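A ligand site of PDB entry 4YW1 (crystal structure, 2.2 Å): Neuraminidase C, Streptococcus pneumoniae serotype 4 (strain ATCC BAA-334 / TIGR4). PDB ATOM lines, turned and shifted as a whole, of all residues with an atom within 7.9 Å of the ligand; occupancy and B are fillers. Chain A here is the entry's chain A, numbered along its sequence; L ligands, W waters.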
ATOM      1  N   GLY A  45      14.728  25.602 -14.484  1.00  0.00           N
ATOM      2  CA  GLY A  45      13.382  25.228 -14.877  1.00  0.00           C
ATOM      3  C   GLY A  45      13.353  24.034 -15.805  1.00  0.00           C
ATOM      4  O   GLY A  45      14.385  23.499 -16.232  1.00  0.00           O
ATOM      5  N   LEU A  46      12.132  23.605 -16.111  1.00  0.00           N
ATOM      6  CA  LEU A  46      11.888  22.499 -17.004  1.00  0.00           C
ATOM      7  C   LEU A  46      11.900  23.023 -18.440  1.00  0.00           C
ATOM      8  O   LEU A  46      11.105  23.890 -18.792  1.00  0.00           O
ATOM      9  CB  LEU A  46      10.545  21.839 -16.664  1.00  0.00           C
ATOM     10  CG  LEU A  46      10.149  20.640 -17.516  1.00  0.00           C
ATOM     11  CD1 LEU A  46      11.183  19.534 -17.412  1.00  0.00           C
ATOM     12  CD2 LEU A  46       8.773  20.138 -17.127  1.00  0.00           C
ATOM     13  N   GLN A  47      12.791  22.503 -19.273  1.00  0.00           N
ATOM     14  CA  GLN A  47      13.009  23.020 -20.628  1.00  0.00           C
ATOM     15  C   GLN A  47      12.891  21.945 -21.680  1.00  0.00           C
ATOM     16  O   GLN A  47      13.549  20.895 -21.596  1.00  0.00           O
ATOM     17  CB  GLN A  47      14.391  23.628 -20.733  1.00  0.00           C
ATOM     18  CG  GLN A  47      14.597  24.835 -19.840  1.00  0.00           C
ATOM     19  CD  GLN A  47      15.960  25.441 -20.035  1.00  0.00           C
ATOM     20  OE1 GLN A  47      16.513  25.411 -21.153  1.00  0.00           O
ATOM     21  NE2 GLN A  47      16.517  26.017 -18.969  1.00  0.00           N
ATOM     22  N   GLN A  60      -4.110  20.585 -23.871  1.00  0.00           N
ATOM     23  CA  GLN A  60      -2.806  20.833 -23.292  1.00  0.00           C
ATOM     24  C   GLN A  60      -2.069  19.536 -22.879  1.00  0.00           C
ATOM     25  O   GLN A  60      -0.848  19.551 -22.776  1.00  0.00           O
ATOM     26  CB  GLN A  60      -2.863  21.884 -22.151  1.00  0.00           C
ATOM     27  CG  GLN A  60      -3.739  21.559 -20.962  1.00  0.00           C
ATOM     28  CD  GLN A  60      -5.223  21.851 -21.180  1.00  0.00           C
ATOM     29  OE1 GLN A  60      -5.648  22.223 -22.265  1.00  0.00           O
ATOM     30  NE2 GLN A  60      -6.011  21.634 -20.154  1.00  0.00           N
ATOM     31  N   ASN A  61      -2.782  18.416 -22.742  1.00  0.00           N
ATOM     32  CA  ASN A  61      -2.171  17.098 -22.490  1.00  0.00           C
ATOM     33  C   ASN A  61      -1.964  16.195 -23.736  1.00  0.00           C
ATOM     34  O   ASN A  61      -1.866  14.959 -23.635  1.00  0.00           O
ATOM     35  CB  ASN A  61      -2.969  16.393 -21.394  1.00  0.00           C
ATOM     36  CG  ASN A  61      -2.934  17.142 -20.067  1.00  0.00           C
ATOM     37  OD1 ASN A  61      -2.045  17.988 -19.824  1.00  0.00           O
ATOM     38  ND2 ASN A  61      -3.865  16.829 -19.205  1.00  0.00           N
ATOM     39  N   TYR A  63       0.771  16.021 -26.329  1.00  0.00           N
ATOM     40  CA  TYR A  63       2.087  16.395 -26.839  1.00  0.00           C
ATOM     41  C   TYR A  63       3.159  15.349 -26.648  1.00  0.00           C
ATOM     42  O   TYR A  63       3.043  14.454 -25.820  1.00  0.00           O
ATOM     43  CB  TYR A  63       2.589  17.707 -26.225  1.00  0.00           C
ATOM     44  CG  TYR A  63       2.859  17.687 -24.737  1.00  0.00           C
ATOM     45  CD1 TYR A  63       1.844  17.977 -23.834  1.00  0.00           C
ATOM     46  CD2 TYR A  63       4.126  17.400 -24.229  1.00  0.00           C
ATOM     47  CE1 TYR A  63       2.067  17.986 -22.463  1.00  0.00           C
ATOM     48  CE2 TYR A  63       4.354  17.395 -22.855  1.00  0.00           C
ATOM     49  CZ  TYR A  63       3.329  17.686 -21.972  1.00  0.00           C
ATOM     50  OH  TYR A  63       3.518  17.715 -20.593  1.00  0.00           O
ATOM     51  N   ASP A  65       7.471  15.619 -26.207  1.00  0.00           N
ATOM     52  CA  ASP A  65       8.680  16.439 -26.081  1.00  0.00           C
ATOM     53  C   ASP A  65       9.848  15.616 -25.558  1.00  0.00           C
ATOM     54  O   ASP A  65       9.665  14.484 -25.102  1.00  0.00           O
ATOM     55  CB  ASP A  65       8.428  17.717 -25.226  1.00  0.00           C
ATOM     56  CG  ASP A  65       8.208  17.450 -23.723  1.00  0.00           C
ATOM     57  OD1 ASP A  65       8.068  16.290 -23.284  1.00  0.00           O
ATOM     58  OD2 ASP A  65       8.129  18.463 -22.952  1.00  0.00           O
ATOM     59  N   PHE A  67      12.792  16.687 -22.765  1.00  0.00           N
ATOM     60  CA  PHE A  67      13.036  17.719 -21.752  1.00  0.00           C
ATOM     61  C   PHE A  67      14.319  17.538 -20.940  1.00  0.00           C
ATOM     62  O   PHE A  67      14.864  16.424 -20.844  1.00  0.00           O
ATOM     63  CB  PHE A  67      11.813  17.851 -20.809  1.00  0.00           C
ATOM     64  CG  PHE A  67      11.562  16.656 -19.934  1.00  0.00           C
ATOM     65  CD1 PHE A  67      12.233  16.488 -18.726  1.00  0.00           C
ATOM     66  CD2 PHE A  67      10.626  15.684 -20.310  1.00  0.00           C
ATOM     67  CE1 PHE A  67      11.972  15.397 -17.916  1.00  0.00           C
ATOM     68  CE2 PHE A  67      10.374  14.588 -19.499  1.00  0.00           C
ATOM     69  CZ  PHE A  67      11.049  14.448 -18.308  1.00  0.00           C
ATOM     70  N   LEU A  68      14.769  18.658 -20.372  1.00  0.00           N
ATOM     71  CA  LEU A  68      15.917  18.748 -19.470  1.00  0.00           C
ATOM     72  C   LEU A  68      15.501  19.450 -18.175  1.00  0.00           C
ATOM     73  O   LEU A  68      14.809  20.481 -18.222  1.00  0.00           O
ATOM     74  CB  LEU A  68      17.028  19.583 -20.102  1.00  0.00           C
ATOM     75  CG  LEU A  68      17.537  19.159 -21.477  1.00  0.00           C
ATOM     76  CD1 LEU A  68      18.521  20.195 -22.003  1.00  0.00           C
ATOM     77  CD2 LEU A  68      18.188  17.789 -21.432  1.00  0.00           C
ATOM     78  N   ARG A  69      15.929  18.916 -17.032  1.00  0.00           N
ATOM     79  CA  ARG A  69      15.776  19.581 -15.745  1.00  0.00           C
ATOM     80  C   ARG A  69      17.093  20.170 -15.256  1.00  0.00           C
ATOM     81  O   ARG A  69      18.178  19.836 -15.784  1.00  0.00           O
ATOM     82  CB  ARG A  69      15.256  18.625 -14.682  1.00  0.00           C
ATOM     83  CG  ARG A  69      13.933  18.000 -15.009  1.00  0.00           C
ATOM     84  CD  ARG A  69      13.499  17.084 -13.887  1.00  0.00           C
ATOM     85  NE  ARG A  69      12.437  16.169 -14.299  1.00  0.00           N
ATOM     86  CZ  ARG A  69      11.135  16.484 -14.328  1.00  0.00           C
ATOM     87  NH1 ARG A  69      10.686  17.696 -13.990  1.00  0.00           N
ATOM     88  NH2 ARG A  69      10.262  15.564 -14.729  1.00  0.00           N
ATOM     89  N   GLU A  73      18.721  15.641 -15.416  1.00  0.00           N
ATOM     90  CA  GLU A  73      17.794  14.609 -15.912  1.00  0.00           C
ATOM     91  C   GLU A  73      17.422  14.892 -17.360  1.00  0.00           C
ATOM     92  O   GLU A  73      17.155  16.035 -17.717  1.00  0.00           O
ATOM     93  CB  GLU A  73      16.515  14.515 -15.057  1.00  0.00           C
ATOM     94  CG  GLU A  73      15.632  13.341 -15.431  1.00  0.00           C
ATOM     95  CD  GLU A  73      14.590  12.987 -14.379  1.00  0.00           C
ATOM     96  OE1 GLU A  73      13.818  13.868 -13.965  1.00  0.00           O
ATOM     97  OE2 GLU A  73      14.525  11.819 -13.954  1.00  0.00           O
ATOM     98  N   GLY A  75      14.647  13.435 -20.086  1.00  0.00           N
ATOM     99  CA  GLY A  75      13.429  12.659 -20.241  1.00  0.00           C
ATOM    100  C   GLY A  75      12.635  12.998 -21.491  1.00  0.00           C
ATOM    101  O   GLY A  75      13.004  13.890 -22.263  1.00  0.00           O
ATOM    102  N   MET A  76      11.541  12.263 -21.684  1.00  0.00           N
ATOM    103  CA  MET A  76      10.584  12.569 -22.730  1.00  0.00           C
ATOM    104  C   MET A  76       9.182  12.356 -22.221  1.00  0.00           C
ATOM    105  O   MET A  76       8.949  11.499 -21.353  1.00  0.00           O
ATOM    106  CB  MET A  76      10.838  11.712 -23.969  1.00  0.00           C
ATOM    107  CG  MET A  76      10.603  10.218 -23.757  1.00  0.00           C
ATOM    108  SD  MET A  76       8.918   9.631 -24.100  1.00  0.00           S
ATOM    109  CE  MET A  76       8.892   9.852 -25.876  1.00  0.00           C
ATOM    110  N   GLU A  77       8.236  13.128 -22.758  1.00  0.00           N
ATOM    111  CA  GLU A  77       6.815  12.868 -22.556  1.00  0.00           C
ATOM    112  C   GLU A  77       6.129  12.539 -23.875  1.00  0.00           C
ATOM    113  O   GLU A  77       6.524  13.015 -24.934  1.00  0.00           O
ATOM    114  CB  GLU A  77       6.101  14.059 -21.908  1.00  0.00           C
ATOM    115  CG  GLU A  77       6.701  14.505 -20.589  1.00  0.00           C
ATOM    116  CD  GLU A  77       5.732  15.330 -19.770  1.00  0.00           C
ATOM    117  OE1 GLU A  77       4.885  14.726 -19.094  1.00  0.00           O
ATOM    118  OE2 GLU A  77       5.822  16.587 -19.806  1.00  0.00           O
ATOM    119  N   ARG A  79       1.956  12.146 -24.544  1.00  0.00           N
ATOM    120  CA  ARG A  79       0.668  12.235 -23.855  1.00  0.00           C
ATOM    121  C   ARG A  79      -0.452  12.449 -24.869  1.00  0.00           C
ATOM    122  O   ARG A  79      -0.233  13.112 -25.888  1.00  0.00           O
ATOM    123  CB  ARG A  79       0.667  13.378 -22.872  1.00  0.00           C
ATOM    124  CG  ARG A  79       1.839  13.367 -21.907  1.00  0.00           C
ATOM    125  CD  ARG A  79       1.804  14.569 -20.987  1.00  0.00           C
ATOM    126  NE  ARG A  79       0.738  14.445 -19.996  1.00  0.00           N
ATOM    127  CZ  ARG A  79       0.374  15.418 -19.156  1.00  0.00           C
ATOM    128  NH1 ARG A  79       0.980  16.604 -19.168  1.00  0.00           N
ATOM    129  NH2 ARG A  79      -0.622  15.196 -18.302  1.00  0.00           N
ATOM    130  N   ASN A  86      -0.566   8.969 -20.501  1.00  0.00           N
ATOM    131  CA  ASN A  86       0.537   9.850 -20.136  1.00  0.00           C
ATOM    132  C   ASN A  86       1.798   9.020 -19.935  1.00  0.00           C
ATOM    133  O   ASN A  86       1.919   8.267 -18.969  1.00  0.00           O
ATOM    134  CB  ASN A  86       0.174  10.629 -18.882  1.00  0.00           C
ATOM    135  CG  ASN A  86      -1.177  11.317 -19.004  1.00  0.00           C
ATOM    136  OD1 ASN A  86      -1.305  12.323 -19.688  1.00  0.00           O
ATOM    137  ND2 ASN A  86      -2.198  10.766 -18.350  1.00  0.00           N
ATOM    138  N   ASN A  87       2.713   9.118 -20.890  1.00  0.00           N
ATOM    139  CA  ASN A  87       3.960   8.397 -20.837  1.00  0.00           C
ATOM    140  C   ASN A  87       5.050   9.378 -20.514  1.00  0.00           C
ATOM    141  O   ASN A  87       5.160  10.437 -21.133  1.00  0.00           O
ATOM    142  CB  ASN A  87       4.249   7.686 -22.163  1.00  0.00           C
ATOM    143  CG  ASN A  87       3.147   6.718 -22.549  1.00  0.00           C
ATOM    144  OD1 ASN A  87       2.879   5.753 -21.849  1.00  0.00           O
ATOM    145  ND2 ASN A  87       2.472   6.996 -23.658  1.00  0.00           N
ATOM    146  N   LEU A  88       5.852   9.028 -19.510  1.00  0.00           N
ATOM    147  CA  LEU A  88       7.066   9.772 -19.172  1.00  0.00           C
ATOM    148  C   LEU A  88       8.187   8.754 -19.001  1.00  0.00           C
ATOM    149  O   LEU A  88       8.067   7.823 -18.226  1.00  0.00           O
ATOM    150  CB  LEU A  88       6.866  10.584 -17.906  1.00  0.00           C
ATOM    151  CG  LEU A  88       7.997  11.577 -17.589  1.00  0.00           C
ATOM    152  CD1 LEU A  88       7.504  12.737 -16.743  1.00  0.00           C
ATOM    153  CD2 LEU A  88       9.179  10.907 -16.895  1.00  0.00           C
ATOM    154  N   SER A  90      12.519   8.648 -18.578  1.00  0.00           N
ATOM    155  CA  SER A  90      13.674   9.494 -18.239  1.00  0.00           C
ATOM    156  C   SER A  90      14.788   8.717 -17.517  1.00  0.00           C
ATOM    157  O   SER A  90      14.609   7.567 -17.120  1.00  0.00           O
ATOM    158  CB  SER A  90      13.202  10.634 -17.339  1.00  0.00           C
ATOM    159  OG  SER A  90      12.759  10.129 -16.085  1.00  0.00           O
ATOM    160  N   ARG A 155       1.134  24.726 -25.802  1.00  0.00           N
ATOM    161  CA  ARG A 155      -0.021  24.275 -25.039  1.00  0.00           C
ATOM    162  C   ARG A 155      -1.035  25.421 -24.906  1.00  0.00           C
ATOM    163  O   ARG A 155      -0.711  26.491 -24.380  1.00  0.00           O
ATOM    164  CB  ARG A 155       0.400  23.796 -23.661  1.00  0.00           C
ATOM    165  CG  ARG A 155       1.500  22.740 -23.676  1.00  0.00           C
ATOM    166  CD  ARG A 155       1.890  22.358 -22.257  1.00  0.00           C
ATOM    167  NE  ARG A 155       0.950  21.417 -21.633  1.00  0.00           N
ATOM    168  CZ  ARG A 155       1.030  20.986 -20.368  1.00  0.00           C
ATOM    169  NH1 ARG A 155       1.969  21.445 -19.546  1.00  0.00           N
ATOM    170  NH2 ARG A 155       0.149  20.095 -19.922  1.00  0.00           N
ATOM    171  N   ALA A 160       5.133  26.598 -23.579  1.00  0.00           N
ATOM    172  CA  ALA A 160       5.522  25.981 -22.302  1.00  0.00           C
ATOM    173  C   ALA A 160       6.939  25.396 -22.403  1.00  0.00           C
ATOM    174  O   ALA A 160       7.455  25.103 -23.490  1.00  0.00           O
ATOM    175  CB  ALA A 160       4.521  24.897 -21.907  1.00  0.00           C
ATOM    176  N   PHE A 161       7.564  25.266 -21.232  1.00  0.00           N
ATOM    177  CA  PHE A 161       8.873  24.631 -21.079  1.00  0.00           C
ATOM    178  C   PHE A 161       9.932  25.276 -21.962  1.00  0.00           C
ATOM    179  O   PHE A 161      10.698  24.595 -22.647  1.00  0.00           O
ATOM    180  CB  PHE A 161       8.778  23.115 -21.374  1.00  0.00           C
ATOM    181  CG  PHE A 161       7.586  22.426 -20.749  1.00  0.00           C
ATOM    182  CD1 PHE A 161       7.252  22.620 -19.405  1.00  0.00           C
ATOM    183  CD2 PHE A 161       6.787  21.546 -21.514  1.00  0.00           C
ATOM    184  CE1 PHE A 161       6.174  21.971 -18.838  1.00  0.00           C
ATOM    185  CE2 PHE A 161       5.695  20.893 -20.945  1.00  0.00           C
ATOM    186  CZ  PHE A 161       5.397  21.090 -19.604  1.00  0.00           C
HETATM  187  C1  LIG L   1       1.608  19.245 -16.698  1.00  0.00           C
HETATM  188  C2  LIG L   1       2.130  18.509 -15.474  1.00  0.00           C
HETATM  189  C3  LIG L   1       2.386  17.018 -15.756  1.00  0.00           C
HETATM  190  C4  LIG L   1       3.658  16.795 -16.589  1.00  0.00           C
HETATM  191  C5  LIG L   1       4.849  17.483 -15.939  1.00  0.00           C
HETATM  192  C6  LIG L   1       4.552  18.977 -15.727  1.00  0.00           C
HETATM  193  C7  LIG L   1       5.630  19.762 -14.978  1.00  0.00           C
HETATM  194  C8  LIG L   1       5.168  21.171 -14.582  1.00  0.00           C
HETATM  195  C9  LIG L   1       6.307  22.032 -14.040  1.00  0.00           C
HETATM  196  C10 LIG L   1       7.224  16.868 -16.332  1.00  0.00           C
HETATM  197  C11 LIG L   1       8.311  16.639 -17.347  1.00  0.00           C
HETATM  198  N1  LIG L   1       6.021  17.285 -16.792  1.00  0.00           N
HETATM  199  O1  LIG L   1       2.167  20.304 -17.068  1.00  0.00           O
HETATM  200  O2  LIG L   1       0.631  18.774 -17.329  1.00  0.00           O
HETATM  201  O3  LIG L   1       1.153  18.605 -14.436  1.00  0.00           O
HETATM  202  O4  LIG L   1       3.893  15.387 -16.735  1.00  0.00           O
HETATM  203  O5  LIG L   1       3.328  19.130 -14.974  1.00  0.00           O
HETATM  204  O6  LIG L   1       5.969  19.085 -13.767  1.00  0.00           O
HETATM  205  O7  LIG L   1       4.554  21.804 -15.725  1.00  0.00           O
HETATM  206  O8  LIG L   1       7.027  22.631 -15.128  1.00  0.00           O
HETATM  207  O9  LIG L   1       7.444  16.655 -15.147  1.00  0.00           O
HETATM  208  O   HOH W   1      -2.357  20.139 -18.024  1.00  0.00           O
HETATM  209  O   HOH W   2       7.512  24.812 -16.510  1.00  0.00           O
HETATM  210  O   HOH W   3      -1.132  16.939 -16.118  1.00  0.00           O
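The side-chain carboxylate (OE1) of Glu 77 sits at hydrogen-bond distance from an oxygen (O4) of the ligand. The guanidinium group (NH1) of Arg 155 is in salt-bridge range of an oxygen (O1) of the ligand (2.7 Å). The guanidinium group (NH1) of Arg 79 lies within salt-bridge range of an oxygen (O2) of the ligand, at 2.9 Å. NH2 of Arg 69 sits at hydrogen-bond distance from O9 of the ligand (3.1 Å).
OE2 of Glu 77 sits at hydrogen-bond distance from OH of Tyr 63. NE of Arg 155 lies within hydrogen-bond range of O of Gln 60, 2.8 Å away. The guanidinium group of Arg 79 sits at hydrogen-bond distance from the side-chain amide oxygen of Asn 86. The backbone carbonyl oxygen (O) of Tyr 63 is in hydrogen-bond range of the backbone NH (N) of Arg 79 (2.9 Å). The guanidinium group of Arg 155 sits at hydrogen-bond distance from the side-chain amide oxygen of Asn 61, 3.0 Å away. The guanidinium group of Arg 79 is in hydrogen-bond range of the side-chain amide oxygen of Asn 61, 3.4 Å away. N of Phe 67 sits at hydrogen-bond distance from O of Gly 75, 2.8 Å away. The backbone carbonyl oxygen of Glu 77 is in hydrogen-bond range of the backbone NH of Asp 65.
Leu 46 touches the ligand. OD1 of Asn 61 touches O2 of the ligand, 3.7 Å away. Phe 67 touches the ligand. Phe 161 touches the ligand (CE1 to O7, 3.5 Å). Eight residues have an atom within 4 Å of the ligand: Leu 46, Asn 61, Phe 67, Arg 69, Glu 77, Arg 79, Arg 155 and Phe 161. The nearest printed residue that does not touch the ligand is Leu 88 (4.03 Å).
Water W3 bridges O2 of the ligand (2.8 Å) and NH2 of Arg 79 (2.8 Å). Water W1 lies within hydrogen-bond range of OD1 of Asn 61 (2.8 Å), NH2 of Arg 155 (3.1 Å) and O2 of the ligand (3.4 Å).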
